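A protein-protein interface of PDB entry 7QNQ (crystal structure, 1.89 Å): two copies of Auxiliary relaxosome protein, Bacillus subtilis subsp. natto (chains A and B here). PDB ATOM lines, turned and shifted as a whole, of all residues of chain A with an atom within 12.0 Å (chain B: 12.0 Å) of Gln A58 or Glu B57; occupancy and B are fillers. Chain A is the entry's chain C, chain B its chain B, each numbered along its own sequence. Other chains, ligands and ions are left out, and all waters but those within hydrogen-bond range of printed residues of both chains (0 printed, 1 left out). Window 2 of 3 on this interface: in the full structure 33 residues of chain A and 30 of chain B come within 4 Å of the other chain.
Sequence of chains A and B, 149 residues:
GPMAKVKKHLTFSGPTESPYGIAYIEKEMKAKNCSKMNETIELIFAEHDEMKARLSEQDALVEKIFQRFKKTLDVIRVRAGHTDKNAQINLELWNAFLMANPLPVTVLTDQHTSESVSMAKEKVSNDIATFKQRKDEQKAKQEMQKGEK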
ATOM      1  N   SER A  56      14.914 -11.832  37.240  1.00  0.00           N
ATOM      2  CA  SER A  56      15.827 -10.757  37.609  1.00  0.00           C
ATOM      3  C   SER A  56      17.237 -11.026  37.091  1.00  0.00           C
ATOM      4  O   SER A  56      18.067 -10.121  37.045  1.00  0.00           O
ATOM      5  CB  SER A  56      15.854 -10.571  39.129  1.00  0.00           C
ATOM      6  OG  SER A  56      16.742  -9.534  39.506  1.00  0.00           O
ATOM      7  N   GLU A  57      17.504 -12.277  36.707  1.00  0.00           N
ATOM      8  CA  GLU A  57      18.817 -12.619  36.165  1.00  0.00           C
ATOM      9  C   GLU A  57      19.076 -11.896  34.851  1.00  0.00           C
ATOM     10  O   GLU A  57      20.178 -11.384  34.621  1.00  0.00           O
ATOM     11  CB  GLU A  57      18.929 -14.129  35.966  1.00  0.00           C
ATOM     12  CG  GLU A  57      18.835 -14.930  37.249  1.00  0.00           C
ATOM     13  CD  GLU A  57      19.917 -14.555  38.241  1.00  0.00           C
ATOM     14  OE1 GLU A  57      21.026 -14.178  37.803  1.00  0.00           O
ATOM     15  OE2 GLU A  57      19.659 -14.632  39.462  1.00  0.00           O
ATOM     16  N   GLN A  58      18.072 -11.862  33.973  1.00  0.00           N
ATOM     17  CA  GLN A  58      18.200 -11.123  32.723  1.00  0.00           C
ATOM     18  C   GLN A  58      18.340  -9.629  32.982  1.00  0.00           C
ATOM     19  O   GLN A  58      19.142  -8.951  32.330  1.00  0.00           O
ATOM     20  CB  GLN A  58      16.995 -11.404  31.826  1.00  0.00           C
ATOM     21  CG  GLN A  58      17.234 -12.488  30.791  1.00  0.00           C
ATOM     22  CD  GLN A  58      16.026 -12.727  29.913  1.00  0.00           C
ATOM     23  OE1 GLN A  58      14.998 -12.066  30.058  1.00  0.00           O
ATOM     24  NE2 GLN A  58      16.143 -13.682  28.998  1.00  0.00           N
ATOM     25  N   ASP A  59      17.565  -9.104  33.938  1.00  0.00           N
ATOM     26  CA  ASP A  59      17.592  -7.673  34.232  1.00  0.00           C
ATOM     27  C   ASP A  59      18.966  -7.219  34.712  1.00  0.00           C
ATOM     28  O   ASP A  59      19.408  -6.111  34.384  1.00  0.00           O
ATOM     29  CB  ASP A  59      16.524  -7.338  35.273  1.00  0.00           C
ATOM     30  CG  ASP A  59      15.115  -7.487  34.734  1.00  0.00           C
ATOM     31  OD1 ASP A  59      14.158  -7.331  35.523  1.00  0.00           O
ATOM     32  OD2 ASP A  59      14.962  -7.804  33.535  1.00  0.00           O
ATOM     33  N   ALA A  60      19.645  -8.048  35.510  1.00  0.00           N
ATOM     34  CA  ALA A  60      20.994  -7.700  35.950  1.00  0.00           C
ATOM     35  C   ALA A  60      21.953  -7.610  34.768  1.00  0.00           C
ATOM     36  O   ALA A  60      22.824  -6.731  34.729  1.00  0.00           O
ATOM     37  CB  ALA A  60      21.493  -8.720  36.974  1.00  0.00           C
ATOM     38  N   LEU A  61      21.816  -8.518  33.800  1.00  0.00           N
ATOM     39  CA  LEU A  61      22.631  -8.446  32.592  1.00  0.00           C
ATOM     40  C   LEU A  61      22.253  -7.238  31.741  1.00  0.00           C
ATOM     41  O   LEU A  61      23.132  -6.526  31.242  1.00  0.00           O
ATOM     42  CB  LEU A  61      22.484  -9.735  31.789  1.00  0.00           C
ATOM     43  CG  LEU A  61      23.079  -9.707  30.382  1.00  0.00           C
ATOM     44  CD1 LEU A  61      24.592  -9.556  30.443  1.00  0.00           C
ATOM     45  CD2 LEU A  61      22.688 -10.961  29.625  1.00  0.00           C
ATOM     46  N   VAL A  62      20.950  -6.995  31.565  1.00  0.00           N
ATOM     47  CA  VAL A  62      20.495  -5.842  30.793  1.00  0.00           C
ATOM     48  C   VAL A  62      21.034  -4.554  31.401  1.00  0.00           C
ATOM     49  O   VAL A  62      21.513  -3.665  30.689  1.00  0.00           O
ATOM     50  CB  VAL A  62      18.957  -5.832  30.707  1.00  0.00           C
ATOM     51  CG1 VAL A  62      18.453  -4.509  30.152  1.00  0.00           C
ATOM     52  CG2 VAL A  62      18.464  -6.984  29.846  1.00  0.00           C
ATOM     53  N   GLU A  63      20.983  -4.443  32.729  1.00  0.00           N
ATOM     54  CA  GLU A  63      21.525  -3.264  33.392  1.00  0.00           C
ATOM     55  C   GLU A  63      23.032  -3.154  33.184  1.00  0.00           C
ATOM     56  O   GLU A  63      23.563  -2.047  33.044  1.00  0.00           O
ATOM     57  CB  GLU A  63      21.177  -3.284  34.879  1.00  0.00           C
ATOM     58  CG  GLU A  63      21.438  -1.963  35.583  1.00  0.00           C
ATOM     59  CD  GLU A  63      20.635  -0.813  34.997  1.00  0.00           C
ATOM     60  OE1 GLU A  63      19.509  -1.046  34.500  1.00  0.00           O
ATOM     61  OE2 GLU A  63      21.136   0.329  35.032  1.00  0.00           O
ATOM     62  N   LYS A  64      23.743  -4.286  33.186  1.00  0.00           N
ATOM     63  CA  LYS A  64      25.181  -4.239  32.925  1.00  0.00           C
ATOM     64  C   LYS A  64      25.485  -3.731  31.524  1.00  0.00           C
ATOM     65  O   LYS A  64      26.452  -2.988  31.324  1.00  0.00           O
ATOM     66  CB  LYS A  64      25.837  -5.608  33.105  1.00  0.00           C
ATOM     67  CG  LYS A  64      26.401  -5.879  34.477  1.00  0.00           C
ATOM     68  CD  LYS A  64      27.219  -7.158  34.443  1.00  0.00           C
ATOM     69  CE  LYS A  64      27.801  -7.510  35.798  1.00  0.00           C
ATOM     70  NZ  LYS A  64      28.830  -8.584  35.661  1.00  0.00           N
ATOM     71  N   ILE A  65      24.699  -4.151  30.534  1.00  0.00           N
ATOM     72  CA  ILE A  65      24.942  -3.708  29.164  1.00  0.00           C
ATOM     73  C   ILE A  65      24.781  -2.195  29.063  1.00  0.00           C
ATOM     74  O   ILE A  65      25.628  -1.503  28.486  1.00  0.00           O
ATOM     75  CB  ILE A  65      24.017  -4.451  28.186  1.00  0.00           C
ATOM     76  CG1 ILE A  65      24.365  -5.940  28.169  1.00  0.00           C
ATOM     77  CG2 ILE A  65      24.143  -3.870  26.782  1.00  0.00           C
ATOM     78  CD1 ILE A  65      23.334  -6.800  27.475  1.00  0.00           C
ATOM     79  N   PHE A  66      23.711  -1.656  29.654  1.00  0.00           N
ATOM     80  CA  PHE A  66      23.484  -0.215  29.602  1.00  0.00           C
ATOM     81  C   PHE A  66      24.618   0.550  30.270  1.00  0.00           C
ATOM     82  O   PHE A  66      25.090   1.561  29.738  1.00  0.00           O
ATOM     83  CB  PHE A  66      22.160   0.141  30.271  1.00  0.00           C
ATOM     84  CG  PHE A  66      21.805   1.597  30.159  1.00  0.00           C
ATOM     85  CD1 PHE A  66      21.950   2.441  31.251  1.00  0.00           C
ATOM     86  CD2 PHE A  66      21.405   2.141  28.949  1.00  0.00           C
ATOM     87  CE1 PHE A  66      21.651   3.790  31.156  1.00  0.00           C
ATOM     88  CE2 PHE A  66      21.094   3.489  28.846  1.00  0.00           C
ATOM     89  CZ  PHE A  66      21.223   4.314  29.953  1.00  0.00           C
ATOM     90  N   GLN A  67      25.068   0.084  31.441  1.00  0.00           N
ATOM     91  CA  GLN A  67      26.136   0.780  32.151  1.00  0.00           C
ATOM     92  C   GLN A  67      27.424   0.797  31.341  1.00  0.00           C
ATOM     93  O   GLN A  67      28.202   1.752  31.432  1.00  0.00           O
ATOM     94  CB  GLN A  67      26.376   0.143  33.519  1.00  0.00           C
ATOM     95  CG  GLN A  67      25.264   0.408  34.521  1.00  0.00           C
ATOM     96  CD  GLN A  67      24.982   1.891  34.693  1.00  0.00           C
ATOM     97  OE1 GLN A  67      23.839   2.330  34.577  1.00  0.00           O
ATOM     98  NE2 GLN A  67      26.032   2.675  34.932  1.00  0.00           N
ATOM     99  N   GLU B  57      12.353 -16.304  24.283  1.00  0.00           N
ATOM    100  CA  GLU B  57      13.583 -16.739  24.935  1.00  0.00           C
ATOM    101  C   GLU B  57      14.723 -15.748  24.681  1.00  0.00           C
ATOM    102  O   GLU B  57      14.879 -14.767  25.409  1.00  0.00           O
ATOM    103  CB  GLU B  57      13.971 -18.137  24.449  1.00  0.00           C
ATOM    104  CG  GLU B  57      15.165 -18.743  25.172  1.00  0.00           C
ATOM    105  CD  GLU B  57      15.623 -20.049  24.549  1.00  0.00           C
ATOM    106  OE1 GLU B  57      14.942 -20.534  23.622  1.00  0.00           O
ATOM    107  OE2 GLU B  57      16.661 -20.588  24.986  1.00  0.00           O
ATOM    108  N   GLN B  58      15.526 -16.032  23.650  1.00  0.00           N
ATOM    109  CA  GLN B  58      16.591 -15.122  23.240  1.00  0.00           C
ATOM    110  C   GLN B  58      16.030 -13.780  22.781  1.00  0.00           C
ATOM    111  O   GLN B  58      16.566 -12.715  23.122  1.00  0.00           O
ATOM    112  CB  GLN B  58      17.405 -15.771  22.125  1.00  0.00           C
ATOM    113  CG  GLN B  58      18.751 -15.115  21.871  1.00  0.00           C
ATOM    114  CD  GLN B  58      19.548 -15.841  20.805  1.00  0.00           C
ATOM    115  OE1 GLN B  58      19.129 -15.947  19.649  1.00  0.00           O
ATOM    116  NE2 GLN B  58      20.699 -16.366  21.197  1.00  0.00           N
ATOM    117  N   ASP B  59      14.945 -13.817  22.009  1.00  0.00           N
ATOM    118  CA  ASP B  59      14.351 -12.592  21.498  1.00  0.00           C
ATOM    119  C   ASP B  59      13.815 -11.721  22.624  1.00  0.00           C
ATOM    120  O   ASP B  59      13.898 -10.489  22.558  1.00  0.00           O
ATOM    121  CB  ASP B  59      13.252 -12.933  20.496  1.00  0.00           C
ATOM    122  CG  ASP B  59      13.800 -13.542  19.220  1.00  0.00           C
ATOM    123  OD1 ASP B  59      15.038 -13.689  19.105  1.00  0.00           O
ATOM    124  OD2 ASP B  59      12.992 -13.885  18.331  1.00  0.00           O
ATOM    125  N   ALA B  60      13.250 -12.343  23.661  1.00  0.00           N
ATOM    126  CA  ALA B  60      12.763 -11.581  24.806  1.00  0.00           C
ATOM    127  C   ALA B  60      13.898 -10.832  25.493  1.00  0.00           C
ATOM    128  O   ALA B  60      13.710  -9.709  25.976  1.00  0.00           O
ATOM    129  CB  ALA B  60      12.052 -12.508  25.792  1.00  0.00           C
ATOM    130  N   LEU B  61      15.082 -11.446  25.559  1.00  0.00           N
ATOM    131  CA  LEU B  61      16.236 -10.755  26.122  1.00  0.00           C
ATOM    132  C   LEU B  61      16.651  -9.583  25.242  1.00  0.00           C
ATOM    133  O   LEU B  61      16.924  -8.487  25.744  1.00  0.00           O
ATOM    134  CB  LEU B  61      17.401 -11.730  26.288  1.00  0.00           C
ATOM    135  CG  LEU B  61      18.754 -11.095  26.614  1.00  0.00           C
ATOM    136  CD1 LEU B  61      18.718 -10.429  27.984  1.00  0.00           C
ATOM    137  CD2 LEU B  61      19.877 -12.125  26.531  1.00  0.00           C
ATOM    138  N   VAL B  62      16.700  -9.799  23.925  1.00  0.00           N
ATOM    139  CA  VAL B  62      17.071  -8.740  22.991  1.00  0.00           C
ATOM    140  C   VAL B  62      16.093  -7.571  23.084  1.00  0.00           C
ATOM    141  O   VAL B  62      16.502  -6.402  23.097  1.00  0.00           O
ATOM    142  CB  VAL B  62      17.163  -9.305  21.560  1.00  0.00           C
ATOM    143  CG1 VAL B  62      17.311  -8.180  20.542  1.00  0.00           C
ATOM    144  CG2 VAL B  62      18.320 -10.285  21.452  1.00  0.00           C
ATOM    145  N   GLU B  63      14.790  -7.865  23.149  1.00  0.00           N
ATOM    146  CA  GLU B  63      13.793  -6.807  23.287  1.00  0.00           C
ATOM    147  C   GLU B  63      13.949  -6.067  24.610  1.00  0.00           C
ATOM    148  O   GLU B  63      13.772  -4.843  24.670  1.00  0.00           O
ATOM    149  CB  GLU B  63      12.384  -7.389  23.157  1.00  0.00           C
ATOM    150  CG  GLU B  63      11.284  -6.343  23.011  1.00  0.00           C
ATOM    151  CD  GLU B  63      11.449  -5.467  21.777  1.00  0.00           C
ATOM    152  OE1 GLU B  63      11.995  -5.946  20.760  1.00  0.00           O
ATOM    153  OE2 GLU B  63      11.032  -4.289  21.829  1.00  0.00           O
ATOM    154  N   LYS B  64      14.268  -6.792  25.683  1.00  0.00           N
ATOM    155  CA  LYS B  64      14.506  -6.144  26.968  1.00  0.00           C
ATOM    156  C   LYS B  64      15.693  -5.196  26.897  1.00  0.00           C
ATOM    157  O   LYS B  64      15.668  -4.117  27.501  1.00  0.00           O
ATOM    158  CB  LYS B  64      14.733  -7.187  28.063  1.00  0.00           C
ATOM    159  CG  LYS B  64      13.483  -7.612  28.810  1.00  0.00           C
ATOM    160  CD  LYS B  64      13.832  -8.570  29.944  1.00  0.00           C
ATOM    161  CE  LYS B  64      12.593  -9.050  30.686  1.00  0.00           C
ATOM    162  NZ  LYS B  64      12.959  -9.776  31.934  1.00  0.00           N
ATOM    163  N   ILE B  65      16.752  -5.593  26.188  1.00  0.00           N
ATOM    164  CA  ILE B  65      17.926  -4.733  26.063  1.00  0.00           C
ATOM    165  C   ILE B  65      17.558  -3.441  25.344  1.00  0.00           C
ATOM    166  O   ILE B  65      17.869  -2.339  25.810  1.00  0.00           O
ATOM    167  CB  ILE B  65      19.058  -5.472  25.330  1.00  0.00           C
ATOM    168  CG1 ILE B  65      19.575  -6.651  26.151  1.00  0.00           C
ATOM    169  CG2 ILE B  65      20.202  -4.523  25.022  1.00  0.00           C
ATOM    170  CD1 ILE B  65      20.490  -7.565  25.357  1.00  0.00           C
ATOM    171  N   PHE B  66      16.851  -3.557  24.219  1.00  0.00           N
ATOM    172  CA  PHE B  66      16.489  -2.366  23.461  1.00  0.00           C
ATOM    173  C   PHE B  66      15.617  -1.434  24.289  1.00  0.00           C
ATOM    174  O   PHE B  66      15.837  -0.219  24.305  1.00  0.00           O
ATOM    175  CB  PHE B  66      15.770  -2.754  22.171  1.00  0.00           C
ATOM    176  CG  PHE B  66      15.499  -1.586  21.269  1.00  0.00           C
ATOM    177  CD1 PHE B  66      16.529  -0.999  20.552  1.00  0.00           C
ATOM    178  CD2 PHE B  66      14.230  -1.032  21.191  1.00  0.00           C
ATOM    179  CE1 PHE B  66      16.291   0.087  19.731  1.00  0.00           C
ATOM    180  CE2 PHE B  66      13.985   0.059  20.377  1.00  0.00           C
ATOM    181  CZ  PHE B  66      15.018   0.620  19.646  1.00  0.00           C
ATOM    182  N   GLN B  67      14.634  -1.991  25.004  1.00  0.00           N
ATOM    183  CA  GLN B  67      13.743  -1.166  25.813  1.00  0.00           C
ATOM    184  C   GLN B  67      14.498  -0.427  26.911  1.00  0.00           C
ATOM    185  O   GLN B  67      14.101   0.679  27.296  1.00  0.00           O
ATOM    186  CB  GLN B  67      12.631  -2.026  26.416  1.00  0.00           C
ATOM    187  CG  GLN B  67      11.606  -2.500  25.399  1.00  0.00           C
ATOM    188  CD  GLN B  67      10.955  -1.358  24.642  1.00  0.00           C
ATOM    189  OE1 GLN B  67      10.616  -0.324  25.224  1.00  0.00           O
ATOM    190  NE2 GLN B  67      10.776  -1.539  23.338  1.00  0.00           N
ATOM    191  N   ARG B  68      15.569  -1.023  27.442  1.00  0.00           N
ATOM    192  CA  ARG B  68      16.372  -0.322  28.440  1.00  0.00           C
ATOM    193  C   ARG B  68      17.058   0.904  27.847  1.00  0.00           C
ATOM    194  O   ARG B  68      17.241   1.910  28.543  1.00  0.00           O
ATOM    195  CB  ARG B  68      17.398  -1.276  29.049  1.00  0.00           C
ATOM    196  CG  ARG B  68      18.322  -0.647  30.078  1.00  0.00           C
ATOM    197  CD  ARG B  68      17.523  -0.059  31.223  1.00  0.00           C
ATOM    198  NE  ARG B  68      18.373   0.567  32.233  1.00  0.00           N
ATOM    199  CZ  ARG B  68      18.677   1.861  32.260  1.00  0.00           C
ATOM    200  NH1 ARG B  68      18.211   2.675  31.321  1.00  0.00           N
ATOM    201  NH2 ARG B  68      19.448   2.340  33.226  1.00  0.00           N
ATOM    202  N   PHE B  69      17.421   0.847  26.567  1.00  0.00           N
ATOM    203  CA  PHE B  69      18.098   1.938  25.875  1.00  0.00           C
ATOM    204  C   PHE B  69      17.148   2.956  25.250  1.00  0.00           C
ATOM    205  O   PHE B  69      17.595   4.057  24.898  1.00  0.00           O
ATOM    206  CB  PHE B  69      18.992   1.370  24.764  1.00  0.00           C
ATOM    207  CG  PHE B  69      20.304   0.815  25.249  1.00  0.00           C
ATOM    208  CD1 PHE B  69      20.356  -0.362  25.981  1.00  0.00           C
ATOM    209  CD2 PHE B  69      21.494   1.452  24.930  1.00  0.00           C
ATOM    210  CE1 PHE B  69      21.568  -0.872  26.410  1.00  0.00           C
ATOM    211  CE2 PHE B  69      22.711   0.945  25.356  1.00  0.00           C
ATOM    212  CZ  PHE B  69      22.745  -0.221  26.098  1.00  0.00           C
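No residue of chain B comes within 4 Å of Ser A56.
Glu A57 touches none of the printed residues of chain B.
Gln A58 touches just these residues of chain B: Glu B57, Leu B61 and Lys B64.
No residue of chain B comes within 4 Å of Ala A60.
No residue of chain B comes within 4 Å of Leu A61.
Val A62 touches just these residues of chain B: Leu B61, Lys B64, Ile B65 and Arg B68.
Lys A64 touches none of the printed residues of chain B.
Of the printed residues of chain B, Ile A65 touches Ile B65 (3.6 Å) and Phe B69 (3.96 Å).
Printed residues of chain B within 4 Å of Phe A66: Arg B68 and Phe B69.
Glu B57 touches just one residue of chain A: Gln A58.
Gln B58 touches none of the printed residues of chain A.
No residue of chain A comes within 4 Å of Asp B59.
Glu B63 touches none of the printed residues of chain A.
Of chain A, only Gln A58, Asp A59 and Val A62 come within 4 Å of Lys B64.
Of the printed residues of chain A, Ile B65 touches Val A62 (3.9 Å) and Ile A65 (3.6 Å).
Of the printed residues of chain A, Arg B68 touches Val A62, Glu A63 and Phe A66.
The nearest printed residue of chain A that does not touch Glu B57 is Val A62 (9.6 Å).
The side-chain carboxylate of Glu A63 sits close to the side-chain amide oxygen of Gln A67 (3.4 Å).
Among the printed residues, merely in contact across the chains: Phe A66 with Arg B68 (3.2 Å), Gln A58 with Leu B61 (3.6 Å), Val A62 with Arg B68 (3.6 Å), Phe A66 with Phe B69 (3.6 Å), Gln A58 with Lys B64 (3.6 Å), Ile A65 with Ile B65 (3.6 Å), Val A62 with Lys B64 (3.9 Å), Val A62 with Ile B65 (3.9 Å), Val A62 with Leu B61 (3.9 Å), Gln A58 with Glu B57 (3.96 Å) and Ile A65 with Phe B69 (3.96 Å).
Hydrophobic or aromatic side chains of chain B that line the printed part of chain A: Leu B61, Ile B65 and Phe B69.
The side-chain carboxylate (OD2) of Asp A59 lies within salt-bridge range of the side-chain amino group (NZ) of Lys B64 (3.2 Å).
NE of Arg B68 is in salt-bridge range of OE1 of Glu A63 (3.0 Å).
Gln A58 touches Glu B57, but with the chains exchanged Glu A57 does not touch Gln B58 (12.0 Å).
Gln A58 touches Leu B61, but with the chains exchanged Leu A61 does not touch Gln B58 (9.1 Å).
Val A62 touches Leu B61, but with the chains exchanged Leu A61 does not touch Val B62 (8.3 Å).
Ile A65 touches its own counterpart, Ile B65.
Positions printed for both chains: 57, 58, 59, 60, 61, 62, 63, 64, 65, 66 and 67.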
